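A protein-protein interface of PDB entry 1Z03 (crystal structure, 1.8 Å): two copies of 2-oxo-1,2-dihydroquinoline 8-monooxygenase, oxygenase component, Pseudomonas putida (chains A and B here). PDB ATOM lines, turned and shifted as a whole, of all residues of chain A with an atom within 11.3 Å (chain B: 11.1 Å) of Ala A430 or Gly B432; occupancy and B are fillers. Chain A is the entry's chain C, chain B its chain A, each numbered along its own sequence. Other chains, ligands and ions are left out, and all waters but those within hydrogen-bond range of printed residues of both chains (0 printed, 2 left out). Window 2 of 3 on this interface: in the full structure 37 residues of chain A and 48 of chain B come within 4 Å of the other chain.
The guanidinium group of Arg B434 lies within salt-bridge range of the side-chain carboxylate of Asp A431, 2.7 Å away.
Of chain B, only Thr B429, Gly B432, Lys B433 and Arg B434 come within 4 Å of Ala A430.
Thr A429 touches just one residue of chain B: Thr B429.
Asp A431 touches just one residue of chain B: Arg B434 (2.7 Å).
No residue of chain B comes within 4 Å of Gly A432.
Of chain A, only Phe A426 (3.5 Å), Thr A429 (3.7 Å) and Ala A430 (3.5 Å) come within 4 Å of Thr B429.
No residue of chain A comes within 4 Å of Ala B430.
Of the printed residues of chain A, Pro B435 touches Ser A423 and Phe A426.
Printed residues of chain B within 4 Å of Leu A424: Phe B206.
Of the printed residues of chain A, Phe B206 touches Ser A423 (3.9 Å), Leu A424 (3.7 Å) and Lys A427 (3.5 Å).
Thr A422 touches none of the printed residues of chain B.
Lys B427 touches none of the printed residues of chain A.
The nearest residue of chain B that does not touch Ala A430 is Pro B435 (5.3 Å).
The nearest residue of chain A that does not touch Gly B432 is Asp A431 (5.2 Å).
The nearest printed residue of chain B that does not touch Phe A426 is Arg B434 (5.1 Å).
OE2 of Glu B440 is in salt-bridge range of NZ of Lys B433 (3.0 Å).
The backbone carbonyl oxygen (O) of Ile B425 lies within hydrogen-bond range of the side-chain hydroxyl (OG1) of Thr B429.
O of Ile A425 sits at hydrogen-bond distance from OG1 of Thr A429 (2.7 Å).
The backbone carbonyl oxygen of Gln B428 sits at hydrogen-bond distance from the backbone NH of Lys B433 (2.9 Å).
Printed residues of chain B that touch a printed residue of chain A: Phe B206, Ile B425, Phe B426, Thr B429, Gly B432, Lys B433, Arg B434 and Pro B435.
Hydrophobic or aromatic side chains of chain A within 4 Å of the printed part of chain B: Leu A424, Phe A426 and Ala A430.
Phe B206 touches Ser A423.
Ser A423 touches Pro B435 (O to CG, 3.9 Å).
CD2 of Leu A424 touches O of Phe B206, 3.7 Å away.
CE2 of Phe A426 touches CE2 of Phe B426 (3.8 Å).
CB of Phe A426 touches CG of Pro B435 (3.97 Å).
CD1 of Phe B206 touches CD of Lys A427, 3.5 Å away.
CE of Lys A427 touches NH1 of Arg B434 (3.5 Å).
Thr A429 touches Thr B429 (CG2 to CG2, 3.7 Å).
CB of Ala A430 touches O of Lys B433, at 3.7 Å.
N of Arg B434 touches CB of Ala A430, at 3.8 Å.
Phe A426 touches Ile B425, but with the chains exchanged Ile A425 does not touch Phe B426 (7.4 Å).
Phe B426 touches its own counterpart, Phe A426.
Ala A430 touches Thr B429, but with the chains exchanged Thr A429 does not touch Ala B430 (5.9 Å).
Asp A431 touches Arg B434, but with the chains exchanged Arg A434 does not touch Asp B431 (13.0 Å).
Of the 15 pairs that touch across the chains among the printed residues, 2 have their exchanged pair printed and touching as well.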
ATOM      1  N   LYS A 420      -8.601  21.067  -6.473  1.00  0.00           N
ATOM      2  CA  LYS A 420      -8.960  21.896  -5.333  1.00  0.00           C
ATOM      3  C   LYS A 420      -9.239  21.219  -4.006  1.00  0.00           C
ATOM      4  O   LYS A 420      -9.188  21.880  -2.967  1.00  0.00           O
ATOM      5  CB  LYS A 420     -10.171  22.764  -5.691  1.00  0.00           C
ATOM      6  CG  LYS A 420      -9.984  23.581  -6.960  1.00  0.00           C
ATOM      7  CD  LYS A 420     -10.997  24.703  -7.053  1.00  0.00           C
ATOM      8  CE  LYS A 420     -11.031  25.311  -8.449  1.00  0.00           C
ATOM      9  NZ  LYS A 420      -9.672  25.487  -9.040  1.00  0.00           N
ATOM     10  N   THR A 422      -7.628  18.313  -2.496  1.00  0.00           N
ATOM     11  CA  THR A 422      -6.637  17.312  -2.104  1.00  0.00           C
ATOM     12  C   THR A 422      -6.516  17.225  -0.579  1.00  0.00           C
ATOM     13  O   THR A 422      -6.889  18.167   0.135  1.00  0.00           O
ATOM     14  CB  THR A 422      -5.257  17.663  -2.671  1.00  0.00           C
ATOM     15  OG1 THR A 422      -4.770  18.840  -2.018  1.00  0.00           O
ATOM     16  CG2 THR A 422      -5.348  17.936  -4.167  1.00  0.00           C
ATOM     17  N   SER A 423      -5.994  16.101  -0.083  1.00  0.00           N
ATOM     18  CA  SER A 423      -5.828  15.920   1.356  1.00  0.00           C
ATOM     19  C   SER A 423      -4.785  16.904   1.883  1.00  0.00           C
ATOM     20  O   SER A 423      -4.842  17.304   3.045  1.00  0.00           O
ATOM     21  CB  SER A 423      -5.425  14.481   1.686  1.00  0.00           C
ATOM     22  OG  SER A 423      -4.172  14.158   1.110  1.00  0.00           O
ATOM     23  N   LEU A 424      -3.837  17.291   1.024  1.00  0.00           N
ATOM     24  CA  LEU A 424      -2.807  18.273   1.391  1.00  0.00           C
ATOM     25  C   LEU A 424      -3.459  19.627   1.685  1.00  0.00           C
ATOM     26  O   LEU A 424      -3.075  20.331   2.630  1.00  0.00           O
ATOM     27  CB  LEU A 424      -1.789  18.443   0.257  1.00  0.00           C
ATOM     28  CG  LEU A 424      -0.651  17.419   0.187  1.00  0.00           C
ATOM     29  CD1 LEU A 424       0.095  17.553  -1.132  1.00  0.00           C
ATOM     30  CD2 LEU A 424       0.295  17.632   1.379  1.00  0.00           C
ATOM     31  N   ILE A 425      -4.446  19.993   0.868  1.00  0.00           N
ATOM     32  CA  ILE A 425      -5.163  21.252   1.073  1.00  0.00           C
ATOM     33  C   ILE A 425      -6.013  21.179   2.351  1.00  0.00           C
ATOM     34  O   ILE A 425      -6.050  22.136   3.125  1.00  0.00           O
ATOM     35  CB  ILE A 425      -6.037  21.593  -0.161  1.00  0.00           C
ATOM     36  CG1 ILE A 425      -5.122  22.042  -1.304  1.00  0.00           C
ATOM     37  CG2 ILE A 425      -7.038  22.731   0.161  1.00  0.00           C
ATOM     38  CD1 ILE A 425      -5.817  22.179  -2.650  1.00  0.00           C
ATOM     39  N   PHE A 426      -6.677  20.049   2.597  1.00  0.00           N
ATOM     40  CA  PHE A 426      -7.472  19.927   3.809  1.00  0.00           C
ATOM     41  C   PHE A 426      -6.564  19.967   5.036  1.00  0.00           C
ATOM     42  O   PHE A 426      -6.942  20.519   6.059  1.00  0.00           O
ATOM     43  CB  PHE A 426      -8.318  18.646   3.787  1.00  0.00           C
ATOM     44  CG  PHE A 426      -9.574  18.776   2.965  1.00  0.00           C
ATOM     45  CD1 PHE A 426      -9.689  18.151   1.723  1.00  0.00           C
ATOM     46  CD2 PHE A 426     -10.628  19.572   3.413  1.00  0.00           C
ATOM     47  CE1 PHE A 426     -10.832  18.317   0.933  1.00  0.00           C
ATOM     48  CE2 PHE A 426     -11.777  19.746   2.635  1.00  0.00           C
ATOM     49  CZ  PHE A 426     -11.879  19.119   1.391  1.00  0.00           C
ATOM     50  N   LYS A 427      -5.363  19.396   4.924  1.00  0.00           N
ATOM     51  CA  LYS A 427      -4.408  19.417   6.030  1.00  0.00           C
ATOM     52  C   LYS A 427      -4.042  20.876   6.335  1.00  0.00           C
ATOM     53  O   LYS A 427      -4.109  21.315   7.489  1.00  0.00           O
ATOM     54  CB  LYS A 427      -3.139  18.637   5.656  1.00  0.00           C
ATOM     55  CG  LYS A 427      -1.991  18.782   6.656  1.00  0.00           C
ATOM     56  CD  LYS A 427      -0.627  18.514   6.009  1.00  0.00           C
ATOM     57  CE  LYS A 427       0.505  18.651   7.031  1.00  0.00           C
ATOM     58  NZ  LYS A 427       1.864  18.338   6.467  1.00  0.00           N
ATOM     59  N   GLN A 428      -3.657  21.628   5.307  1.00  0.00           N
ATOM     60  CA  GLN A 428      -3.288  23.028   5.500  1.00  0.00           C
ATOM     61  C   GLN A 428      -4.449  23.840   6.050  1.00  0.00           C
ATOM     62  O   GLN A 428      -4.254  24.677   6.923  1.00  0.00           O
ATOM     63  CB  GLN A 428      -2.817  23.648   4.187  1.00  0.00           C
ATOM     64  CG  GLN A 428      -1.598  22.964   3.606  1.00  0.00           C
ATOM     65  CD  GLN A 428      -1.327  23.381   2.173  1.00  0.00           C
ATOM     66  OE1 GLN A 428      -0.535  22.748   1.475  1.00  0.00           O
ATOM     67  NE2 GLN A 428      -1.983  24.451   1.727  1.00  0.00           N
ATOM     68  N   THR A 429      -5.654  23.591   5.542  1.00  0.00           N
ATOM     69  CA  THR A 429      -6.840  24.312   5.994  1.00  0.00           C
ATOM     70  C   THR A 429      -7.122  23.985   7.454  1.00  0.00           C
ATOM     71  O   THR A 429      -7.486  24.866   8.240  1.00  0.00           O
ATOM     72  CB  THR A 429      -8.066  23.955   5.131  1.00  0.00           C
ATOM     73  OG1 THR A 429      -7.729  24.164   3.754  1.00  0.00           O
ATOM     74  CG2 THR A 429      -9.280  24.832   5.492  1.00  0.00           C
ATOM     75  N   ALA A 430      -6.950  22.717   7.818  1.00  0.00           N
ATOM     76  CA  ALA A 430      -7.170  22.297   9.195  1.00  0.00           C
ATOM     77  C   ALA A 430      -6.196  23.043  10.101  1.00  0.00           C
ATOM     78  O   ALA A 430      -6.546  23.432  11.213  1.00  0.00           O
ATOM     79  CB  ALA A 430      -6.969  20.790   9.325  1.00  0.00           C
ATOM     80  N   ASP A 431      -4.975  23.244   9.610  1.00  0.00           N
ATOM     81  CA  ASP A 431      -3.936  23.945  10.353  1.00  0.00           C
ATOM     82  C   ASP A 431      -4.170  25.457  10.428  1.00  0.00           C
ATOM     83  O   ASP A 431      -3.413  26.178  11.089  1.00  0.00           O
ATOM     84  CB  ASP A 431      -2.577  23.672   9.722  1.00  0.00           C
ATOM     85  CG  ASP A 431      -2.102  22.239   9.942  1.00  0.00           C
ATOM     86  OD1 ASP A 431      -1.027  21.902   9.402  1.00  0.00           O
ATOM     87  OD2 ASP A 431      -2.788  21.462  10.650  1.00  0.00           O
ATOM     88  N   GLY A 432      -5.203  25.932   9.736  1.00  0.00           N
ATOM     89  CA  GLY A 432      -5.533  27.347   9.778  1.00  0.00           C
ATOM     90  C   GLY A 432      -4.972  28.184   8.649  1.00  0.00           C
ATOM     91  O   GLY A 432      -5.104  29.405   8.656  1.00  0.00           O
ATOM     92  N   LYS A 433      -4.365  27.532   7.669  1.00  0.00           N
ATOM     93  CA  LYS A 433      -3.772  28.237   6.542  1.00  0.00           C
ATOM     94  C   LYS A 433      -4.727  28.451   5.380  1.00  0.00           C
ATOM     95  O   LYS A 433      -5.259  27.504   4.822  1.00  0.00           O
ATOM     96  CB  LYS A 433      -2.534  27.485   6.068  1.00  0.00           C
ATOM     97  CG  LYS A 433      -1.509  27.305   7.171  1.00  0.00           C
ATOM     98  CD  LYS A 433      -0.313  26.520   6.687  1.00  0.00           C
ATOM     99  CE  LYS A 433       0.700  26.321   7.805  1.00  0.00           C
ATOM    100  NZ  LYS A 433       1.736  25.314   7.424  1.00  0.00           N
ATOM    101  N   ARG A 434      -4.930  29.715   5.021  1.00  0.00           N
ATOM    102  CA  ARG A 434      -5.817  30.092   3.919  1.00  0.00           C
ATOM    103  C   ARG A 434      -5.127  29.884   2.579  1.00  0.00           C
ATOM    104  O   ARG A 434      -3.910  29.740   2.525  1.00  0.00           O
ATOM    105  CB  ARG A 434      -6.156  31.575   4.009  1.00  0.00           C
ATOM    106  CG  ARG A 434      -6.938  32.025   5.225  1.00  0.00           C
ATOM    107  CD  ARG A 434      -6.998  33.553   5.223  1.00  0.00           C
ATOM    108  NE  ARG A 434      -8.051  34.080   6.081  1.00  0.00           N
ATOM    109  CZ  ARG A 434      -8.440  35.349   6.064  1.00  0.00           C
ATOM    110  NH1 ARG A 434      -9.410  35.764   6.866  1.00  0.00           N
ATOM    111  NH2 ARG A 434      -7.850  36.202   5.236  1.00  0.00           N
ATOM    112  N   PRO A 435      -5.897  29.847   1.479  1.00  0.00           N
ATOM    113  CA  PRO A 435      -5.289  29.677   0.155  1.00  0.00           C
ATOM    114  C   PRO A 435      -4.292  30.843   0.027  1.00  0.00           C
ATOM    115  O   PRO A 435      -4.580  31.955   0.479  1.00  0.00           O
ATOM    116  CB  PRO A 435      -6.475  29.832  -0.787  1.00  0.00           C
ATOM    117  CG  PRO A 435      -7.591  29.215  -0.012  1.00  0.00           C
ATOM    118  CD  PRO A 435      -7.363  29.723   1.410  1.00  0.00           C
ATOM    119  N   GLU A 440       5.389  28.368   0.966  1.00  0.00           N
ATOM    120  CA  GLU A 440       5.970  28.223   2.301  1.00  0.00           C
ATOM    121  C   GLU A 440       7.161  27.269   2.162  1.00  0.00           C
ATOM    122  O   GLU A 440       7.054  26.235   1.506  1.00  0.00           O
ATOM    123  CB  GLU A 440       4.917  27.644   3.251  1.00  0.00           C
ATOM    124  CG  GLU A 440       5.274  27.699   4.726  1.00  0.00           C
ATOM    125  CD  GLU A 440       4.225  27.038   5.620  1.00  0.00           C
ATOM    126  OE1 GLU A 440       4.451  26.986   6.849  1.00  0.00           O
ATOM    127  OE2 GLU A 440       3.181  26.571   5.104  1.00  0.00           O
ATOM    128  N   PHE B 206      -0.076  12.631   4.114  1.00  0.00           N
ATOM    129  CA  PHE B 206      -0.958  13.341   3.205  1.00  0.00           C
ATOM    130  C   PHE B 206      -0.480  13.247   1.769  1.00  0.00           C
ATOM    131  O   PHE B 206       0.486  13.898   1.362  1.00  0.00           O
ATOM    132  CB  PHE B 206      -1.105  14.780   3.691  1.00  0.00           C
ATOM    133  CG  PHE B 206      -1.485  14.859   5.144  1.00  0.00           C
ATOM    134  CD1 PHE B 206      -0.507  15.020   6.120  1.00  0.00           C
ATOM    135  CD2 PHE B 206      -2.796  14.620   5.549  1.00  0.00           C
ATOM    136  CE1 PHE B 206      -0.823  14.931   7.484  1.00  0.00           C
ATOM    137  CE2 PHE B 206      -3.119  14.530   6.907  1.00  0.00           C
ATOM    138  CZ  PHE B 206      -2.128  14.683   7.873  1.00  0.00           C
ATOM    139  N   SER B 423     -19.856  18.132   3.640  1.00  0.00           N
ATOM    140  CA  SER B 423     -19.973  19.134   4.691  1.00  0.00           C
ATOM    141  C   SER B 423     -19.415  18.598   6.008  1.00  0.00           C
ATOM    142  O   SER B 423     -18.975  19.368   6.854  1.00  0.00           O
ATOM    143  CB  SER B 423     -21.434  19.571   4.870  1.00  0.00           C
ATOM    144  OG  SER B 423     -22.267  18.482   5.220  1.00  0.00           O
ATOM    145  N   LEU B 424     -19.451  17.281   6.195  1.00  0.00           N
ATOM    146  CA  LEU B 424     -18.901  16.682   7.411  1.00  0.00           C
ATOM    147  C   LEU B 424     -17.388  16.908   7.435  1.00  0.00           C
ATOM    148  O   LEU B 424     -16.805  17.201   8.481  1.00  0.00           O
ATOM    149  CB  LEU B 424     -19.195  15.179   7.447  1.00  0.00           C
ATOM    150  CG  LEU B 424     -20.536  14.762   8.060  1.00  0.00           C
ATOM    151  CD1 LEU B 424     -20.825  13.280   7.809  1.00  0.00           C
ATOM    152  CD2 LEU B 424     -20.488  15.043   9.553  1.00  0.00           C
ATOM    153  N   ILE B 425     -16.751  16.768   6.274  1.00  0.00           N
ATOM    154  CA  ILE B 425     -15.312  16.974   6.173  1.00  0.00           C
ATOM    155  C   ILE B 425     -14.964  18.452   6.400  1.00  0.00           C
ATOM    156  O   ILE B 425     -13.985  18.754   7.086  1.00  0.00           O
ATOM    157  CB  ILE B 425     -14.777  16.452   4.804  1.00  0.00           C
ATOM    158  CG1 ILE B 425     -14.733  14.913   4.845  1.00  0.00           C
ATOM    159  CG2 ILE B 425     -13.381  17.024   4.510  1.00  0.00           C
ATOM    160  CD1 ILE B 425     -14.485  14.243   3.514  1.00  0.00           C
ATOM    161  N   PHE B 426     -15.754  19.376   5.854  1.00  0.00           N
ATOM    162  CA  PHE B 426     -15.474  20.793   6.095  1.00  0.00           C
ATOM    163  C   PHE B 426     -15.692  21.135   7.577  1.00  0.00           C
ATOM    164  O   PHE B 426     -14.971  21.953   8.134  1.00  0.00           O
ATOM    165  CB  PHE B 426     -16.328  21.697   5.188  1.00  0.00           C
ATOM    166  CG  PHE B 426     -15.787  21.812   3.781  1.00  0.00           C
ATOM    167  CD1 PHE B 426     -16.353  21.097   2.734  1.00  0.00           C
ATOM    168  CD2 PHE B 426     -14.662  22.600   3.520  1.00  0.00           C
ATOM    169  CE1 PHE B 426     -15.811  21.153   1.444  1.00  0.00           C
ATOM    170  CE2 PHE B 426     -14.107  22.666   2.231  1.00  0.00           C
ATOM    171  CZ  PHE B 426     -14.681  21.939   1.191  1.00  0.00           C
ATOM    172  N   LYS B 427     -16.672  20.494   8.213  1.00  0.00           N
ATOM    173  CA  LYS B 427     -16.953  20.713   9.633  1.00  0.00           C
ATOM    174  C   LYS B 427     -15.730  20.318  10.458  1.00  0.00           C
ATOM    175  O   LYS B 427     -15.272  21.073  11.311  1.00  0.00           O
ATOM    176  CB  LYS B 427     -18.153  19.871  10.092  1.00  0.00           C
ATOM    177  CG  LYS B 427     -18.406  19.932  11.606  1.00  0.00           C
ATOM    178  CD  LYS B 427     -19.243  18.754  12.095  1.00  0.00           C
ATOM    179  CE  LYS B 427     -19.487  18.820  13.605  1.00  0.00           C
ATOM    180  NZ  LYS B 427     -20.418  17.761  14.128  1.00  0.00           N
ATOM    181  N   GLN B 428     -15.207  19.123  10.196  1.00  0.00           N
ATOM    182  CA  GLN B 428     -14.039  18.629  10.909  1.00  0.00           C
ATOM    183  C   GLN B 428     -12.817  19.497  10.654  1.00  0.00           C
ATOM    184  O   GLN B 428     -12.056  19.793  11.574  1.00  0.00           O
ATOM    185  CB  GLN B 428     -13.734  17.201  10.484  1.00  0.00           C
ATOM    186  CG  GLN B 428     -14.884  16.246  10.692  1.00  0.00           C
ATOM    187  CD  GLN B 428     -14.585  14.862  10.146  1.00  0.00           C
ATOM    188  OE1 GLN B 428     -15.462  13.997  10.102  1.00  0.00           O
ATOM    189  NE2 GLN B 428     -13.339  14.647   9.727  1.00  0.00           N
ATOM    190  N   THR B 429     -12.636  19.899   9.398  1.00  0.00           N
ATOM    191  CA  THR B 429     -11.504  20.738   9.006  1.00  0.00           C
ATOM    192  C   THR B 429     -11.584  22.100   9.702  1.00  0.00           C
ATOM    193  O   THR B 429     -10.581  22.618  10.197  1.00  0.00           O
ATOM    194  CB  THR B 429     -11.482  20.946   7.477  1.00  0.00           C
ATOM    195  OG1 THR B 429     -11.547  19.671   6.826  1.00  0.00           O
ATOM    196  CG2 THR B 429     -10.204  21.652   7.054  1.00  0.00           C
ATOM    197  N   ALA B 430     -12.781  22.679   9.735  1.00  0.00           N
ATOM    198  CA  ALA B 430     -12.980  23.967  10.383  1.00  0.00           C
ATOM    199  C   ALA B 430     -12.605  23.816  11.851  1.00  0.00           C
ATOM    200  O   ALA B 430     -12.037  24.726  12.457  1.00  0.00           O
ATOM    201  CB  ALA B 430     -14.453  24.406  10.256  1.00  0.00           C
ATOM    202  N   ASP B 431     -12.933  22.660  12.419  1.00  0.00           N
ATOM    203  CA  ASP B 431     -12.641  22.384  13.824  1.00  0.00           C
ATOM    204  C   ASP B 431     -11.145  22.167  14.095  1.00  0.00           C
ATOM    205  O   ASP B 431     -10.737  21.996  15.248  1.00  0.00           O
ATOM    206  CB  ASP B 431     -13.430  21.162  14.293  1.00  0.00           C
ATOM    207  CG  ASP B 431     -14.901  21.464  14.532  1.00  0.00           C
ATOM    208  OD1 ASP B 431     -15.624  20.534  14.939  1.00  0.00           O
ATOM    209  OD2 ASP B 431     -15.337  22.619  14.319  1.00  0.00           O
ATOM    210  N   GLY B 432     -10.340  22.171  13.030  1.00  0.00           N
ATOM    211  CA  GLY B 432      -8.904  21.988  13.164  1.00  0.00           C
ATOM    212  C   GLY B 432      -8.416  20.554  13.002  1.00  0.00           C
ATOM    213  O   GLY B 432      -7.227  20.283  13.201  1.00  0.00           O
ATOM    214  N   LYS B 433      -9.307  19.637  12.629  1.00  0.00           N
ATOM    215  CA  LYS B 433      -8.935  18.226  12.462  1.00  0.00           C
ATOM    216  C   LYS B 433      -8.467  17.838  11.058  1.00  0.00           C
ATOM    217  O   LYS B 433      -9.202  17.960  10.071  1.00  0.00           O
ATOM    218  CB  LYS B 433     -10.103  17.323  12.862  1.00  0.00           C
ATOM    219  CG  LYS B 433     -10.578  17.538  14.288  1.00  0.00           C
ATOM    220  CD  LYS B 433     -11.833  16.734  14.587  1.00  0.00           C
ATOM    221  CE  LYS B 433     -12.349  17.027  15.989  1.00  0.00           C
ATOM    222  NZ  LYS B 433     -13.681  16.395  16.234  1.00  0.00           N
ATOM    223  N   ARG B 434      -7.238  17.348  10.977  1.00  0.00           N
ATOM    224  CA  ARG B 434      -6.658  16.929   9.709  1.00  0.00           C
ATOM    225  C   ARG B 434      -7.213  15.575   9.266  1.00  0.00           C
ATOM    226  O   ARG B 434      -7.806  14.843  10.059  1.00  0.00           O
ATOM    227  CB  ARG B 434      -5.147  16.770   9.850  1.00  0.00           C
ATOM    228  CG  ARG B 434      -4.375  18.010  10.194  1.00  0.00           C
ATOM    229  CD  ARG B 434      -2.977  17.596  10.526  1.00  0.00           C
ATOM    230  NE  ARG B 434      -2.037  18.702  10.440  1.00  0.00           N
ATOM    231  CZ  ARG B 434      -0.719  18.552  10.514  1.00  0.00           C
ATOM    232  NH1 ARG B 434       0.079  19.610  10.422  1.00  0.00           N
ATOM    233  NH2 ARG B 434      -0.196  17.339  10.681  1.00  0.00           N
ATOM    234  N   PRO B 435      -7.036  15.238   7.976  1.00  0.00           N
ATOM    235  CA  PRO B 435      -7.516  13.949   7.473  1.00  0.00           C
ATOM    236  C   PRO B 435      -6.826  12.933   8.388  1.00  0.00           C
ATOM    237  O   PRO B 435      -5.700  13.176   8.827  1.00  0.00           O
ATOM    238  CB  PRO B 435      -6.972  13.922   6.050  1.00  0.00           C
ATOM    239  CG  PRO B 435      -7.079  15.367   5.641  1.00  0.00           C
ATOM    240  CD  PRO B 435      -6.550  16.088   6.873  1.00  0.00           C
ATOM    241  N   GLY B 436      -7.479  11.812   8.684  1.00  0.00           N
ATOM    242  CA  GLY B 436      -6.866  10.852   9.588  1.00  0.00           C
ATOM    243  C   GLY B 436      -6.969   9.382   9.246  1.00  0.00           C
ATOM    244  O   GLY B 436      -7.157   9.003   8.093  1.00  0.00           O
ATOM    245  N   GLU B 440     -12.604   8.498  15.362  1.00  0.00           N
ATOM    246  CA  GLU B 440     -12.856   9.179  16.630  1.00  0.00           C
ATOM    247  C   GLU B 440     -14.200   8.657  17.159  1.00  0.00           C
ATOM    248  O   GLU B 440     -15.159   8.525  16.397  1.00  0.00           O
ATOM    249  CB  GLU B 440     -12.911  10.691  16.378  1.00  0.00           C
ATOM    250  CG  GLU B 440     -12.847  11.563  17.620  1.00  0.00           C
ATOM    251  CD  GLU B 440     -12.998  13.049  17.302  1.00  0.00           C
ATOM    252  OE1 GLU B 440     -13.007  13.864  18.249  1.00  0.00           O
ATOM    253  OE2 GLU B 440     -13.111  13.404  16.106  1.00  0.00           O
